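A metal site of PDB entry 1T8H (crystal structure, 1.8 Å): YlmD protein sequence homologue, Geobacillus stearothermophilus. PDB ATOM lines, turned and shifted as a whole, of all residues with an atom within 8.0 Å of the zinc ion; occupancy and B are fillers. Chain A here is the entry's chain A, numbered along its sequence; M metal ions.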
ATOM      1  N   ALA A 181      12.783   5.993   4.189  1.00  0.00           N
ATOM      2  CA  ALA A 181      13.458   6.787   3.176  1.00  0.00           C
ATOM      3  C   ALA A 181      12.521   6.827   1.980  1.00  0.00           C
ATOM      4  O   ALA A 181      11.456   6.180   2.009  1.00  0.00           O
ATOM      5  CB  ALA A 181      14.782   6.132   2.816  1.00  0.00           C
ATOM      6  N   ILE A 182      12.882   7.549   0.928  1.00  0.00           N
ATOM      7  CA  ILE A 182      11.995   7.624  -0.239  1.00  0.00           C
ATOM      8  C   ILE A 182      12.060   6.308  -1.011  1.00  0.00           C
ATOM      9  O   ILE A 182      13.143   5.759  -1.222  1.00  0.00           O
ATOM     10  CB  ILE A 182      12.347   8.833  -1.141  1.00  0.00           C
ATOM     11  CG1 ILE A 182      11.261   9.024  -2.201  1.00  0.00           C
ATOM     12  CG2 ILE A 182      13.729   8.627  -1.778  1.00  0.00           C
ATOM     13  CD1 ILE A 182      11.285  10.359  -2.891  1.00  0.00           C
ATOM     14  N   GLY A 183      10.907   5.788  -1.411  1.00  0.00           N
ATOM     15  CA  GLY A 183      10.892   4.527  -2.131  1.00  0.00           C
ATOM     16  C   GLY A 183      10.831   4.689  -3.633  1.00  0.00           C
ATOM     17  O   GLY A 183      10.700   5.800  -4.139  1.00  0.00           O
ATOM     18  N   PRO A 184      10.915   3.577  -4.383  1.00  0.00           N
ATOM     19  CA  PRO A 184      10.862   3.673  -5.849  1.00  0.00           C
ATOM     20  C   PRO A 184       9.492   4.167  -6.272  1.00  0.00           C
ATOM     21  O   PRO A 184       9.301   4.648  -7.389  1.00  0.00           O
ATOM     22  CB  PRO A 184      11.145   2.233  -6.291  1.00  0.00           C
ATOM     23  CG  PRO A 184      10.548   1.430  -5.175  1.00  0.00           C
ATOM     24  CD  PRO A 184      10.987   2.184  -3.933  1.00  0.00           C
ATOM     25  N   CYS A 185       8.535   4.060  -5.361  1.00  0.00           N
ATOM     26  CA  CYS A 185       7.183   4.515  -5.602  1.00  0.00           C
ATOM     27  C   CYS A 185       7.167   6.015  -5.916  1.00  0.00           C
ATOM     28  O   CYS A 185       6.301   6.479  -6.656  1.00  0.00           O
ATOM     29  CB  CYS A 185       6.314   4.238  -4.365  1.00  0.00           C
ATOM     30  SG  CYS A 185       7.097   4.665  -2.756  1.00  0.00           S
ATOM     31  N   CYS A 186       8.132   6.763  -5.366  1.00  0.00           N
ATOM     32  CA  CYS A 186       8.185   8.209  -5.556  1.00  0.00           C
ATOM     33  C   CYS A 186       9.536   8.752  -6.071  1.00  0.00           C
ATOM     34  O   CYS A 186       9.631   9.918  -6.439  1.00  0.00           O
ATOM     35  CB  CYS A 186       7.891   8.910  -4.220  1.00  0.00           C
ATOM     36  SG  CYS A 186       6.317   8.516  -3.411  1.00  0.00           S
ATOM     37  N   TYR A 187      10.552   7.909  -6.094  1.00  0.00           N
ATOM     38  CA  TYR A 187      11.882   8.363  -6.517  1.00  0.00           C
ATOM     39  C   TYR A 187      12.276   7.907  -7.914  1.00  0.00           C
ATOM     40  O   TYR A 187      12.615   6.746  -8.116  1.00  0.00           O
ATOM     41  CB  TYR A 187      12.927   7.909  -5.481  1.00  0.00           C
ATOM     42  CG  TYR A 187      14.293   8.550  -5.624  1.00  0.00           C
ATOM     43  CD1 TYR A 187      14.430   9.899  -5.931  1.00  0.00           C
ATOM     44  CD2 TYR A 187      15.446   7.801  -5.391  1.00  0.00           C
ATOM     45  CE1 TYR A 187      15.704  10.506  -5.989  1.00  0.00           C
ATOM     46  CE2 TYR A 187      16.708   8.388  -5.455  1.00  0.00           C
ATOM     47  CZ  TYR A 187      16.829   9.732  -5.751  1.00  0.00           C
ATOM     48  OH  TYR A 187      18.088  10.295  -5.811  1.00  0.00           O
ATOM     49  N   GLU A 243       9.644  -0.523   5.528  1.00  0.00           N
ATOM     50  CA  GLU A 243       8.944  -0.359   4.253  1.00  0.00           C
ATOM     51  C   GLU A 243       8.297   1.018   4.161  1.00  0.00           C
ATOM     52  O   GLU A 243       7.600   1.310   3.183  1.00  0.00           O
ATOM     53  CB  GLU A 243       7.870  -1.435   4.080  1.00  0.00           C
ATOM     54  CG  GLU A 243       8.448  -2.827   3.935  1.00  0.00           C
ATOM     55  CD  GLU A 243       7.401  -3.831   3.534  1.00  0.00           C
ATOM     56  OE1 GLU A 243       6.495  -4.114   4.355  1.00  0.00           O
ATOM     57  OE2 GLU A 243       7.478  -4.319   2.386  1.00  0.00           O
ATOM     58  N   ARG A 244       8.521   1.854   5.163  1.00  0.00           N
ATOM     59  CA  ARG A 244       7.937   3.197   5.160  1.00  0.00           C
ATOM     60  C   ARG A 244       8.621   4.143   4.167  1.00  0.00           C
ATOM     61  O   ARG A 244       9.863   4.245   4.122  1.00  0.00           O
ATOM     62  CB  ARG A 244       8.001   3.815   6.565  1.00  0.00           C
ATOM     63  CG  ARG A 244       7.258   3.057   7.659  1.00  0.00           C
ATOM     64  CD  ARG A 244       7.493   3.737   9.009  1.00  0.00           C
ATOM     65  NE  ARG A 244       6.852   3.040  10.126  1.00  0.00           N
ATOM     66  CZ  ARG A 244       5.577   3.167  10.478  1.00  0.00           C
ATOM     67  NH1 ARG A 244       4.765   3.975   9.812  1.00  0.00           N
ATOM     68  NH2 ARG A 244       5.104   2.474  11.512  1.00  0.00           N
ATOM     69  N   CYS A 245       7.802   4.839   3.377  1.00  0.00           N
ATOM     70  CA  CYS A 245       8.298   5.807   2.399  1.00  0.00           C
ATOM     71  C   CYS A 245       8.044   7.193   2.961  1.00  0.00           C
ATOM     72  O   CYS A 245       6.902   7.506   3.309  1.00  0.00           O
ATOM     73  CB  CYS A 245       7.576   5.670   1.059  1.00  0.00           C
ATOM     74  SG  CYS A 245       7.919   7.047  -0.081  1.00  0.00           S
ATOM     75  N   THR A 246       9.099   7.993   3.066  1.00  0.00           N
ATOM     76  CA  THR A 246       9.015   9.351   3.589  1.00  0.00           C
ATOM     77  C   THR A 246       8.110  10.262   2.770  1.00  0.00           C
ATOM     78  O   THR A 246       7.426  11.125   3.319  1.00  0.00           O
ATOM     79  CB  THR A 246      10.413  10.007   3.666  1.00  0.00           C
ATOM     80  OG1 THR A 246      11.099   9.769   2.441  1.00  0.00           O
ATOM     81  CG2 THR A 246      11.232   9.432   4.850  1.00  0.00           C
ATOM     82  N   SER A 247       8.127  10.079   1.458  1.00  0.00           N
ATOM     83  CA  SER A 247       7.272  10.859   0.586  1.00  0.00           C
ATOM     84  C   SER A 247       5.796  10.439   0.722  1.00  0.00           C
ATOM     85  O   SER A 247       4.901  11.275   0.784  1.00  0.00           O
ATOM     86  CB  SER A 247       7.691  10.678  -0.874  1.00  0.00           C
ATOM     87  OG  SER A 247       6.788  11.341  -1.739  1.00  0.00           O
ATOM     88  N   CYS A 248       5.551   9.132   0.779  1.00  0.00           N
ATOM     89  CA  CYS A 248       4.174   8.649   0.884  1.00  0.00           C
ATOM     90  C   CYS A 248       3.520   8.927   2.223  1.00  0.00           C
ATOM     91  O   CYS A 248       2.354   9.278   2.276  1.00  0.00           O
ATOM     92  CB  CYS A 248       4.128   7.140   0.628  1.00  0.00           C
ATOM     93  SG  CYS A 248       4.404   6.677  -1.086  1.00  0.00           S
ATOM     94  N   GLU A 249       4.267   8.763   3.302  1.00  0.00           N
ATOM     95  CA  GLU A 249       3.711   8.975   4.640  1.00  0.00           C
ATOM     96  C   GLU A 249       3.833  10.406   5.159  1.00  0.00           C
ATOM     97  O   GLU A 249       4.532  10.672   6.122  1.00  0.00           O
ATOM     98  CB  GLU A 249       4.344   7.966   5.606  1.00  0.00           C
ATOM     99  CG  GLU A 249       3.900   6.527   5.272  1.00  0.00           C
ATOM    100  CD  GLU A 249       4.640   5.424   6.015  1.00  0.00           C
ATOM    101  OE1 GLU A 249       4.746   5.485   7.253  1.00  0.00           O
ATOM    102  OE2 GLU A 249       5.111   4.492   5.341  1.00  0.00           O
ATOM    103  N   SER A 255       9.645  15.511   3.678  1.00  0.00           N
ATOM    104  CA  SER A 255      10.127  14.870   2.447  1.00  0.00           C
ATOM    105  C   SER A 255      10.668  15.928   1.531  1.00  0.00           C
ATOM    106  O   SER A 255       9.904  16.765   1.028  1.00  0.00           O
ATOM    107  CB  SER A 255       8.986  14.131   1.732  1.00  0.00           C
ATOM    108  OG  SER A 255       9.424  13.596   0.500  1.00  0.00           O
HETATM  109 ZN    ZN M   1       6.484   6.685  -1.921  1.00  0.00          ZN
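N of Ser 247 sits close to SG of Cys 245, 3.4 Å away.
The side-chain sulfur (SG) of Cys 245 sits close to the backbone NH (N) of Gly 183 (3.5 Å).
The backbone NH of Cys 245 is in hydrogen-bond range of the side-chain carboxylate of Glu 249.
SG of Cys 186 lies close to OG of Ser 247.
The zinc ion is bound by SG of Cys 248 (2.2 Å), SG of Cys 185 (2.3 Å), SG of Cys 245 (2.4 Å) and SG of Cys 186 (2.4 Å).
The zinc ion has four donor atoms within binding distance.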
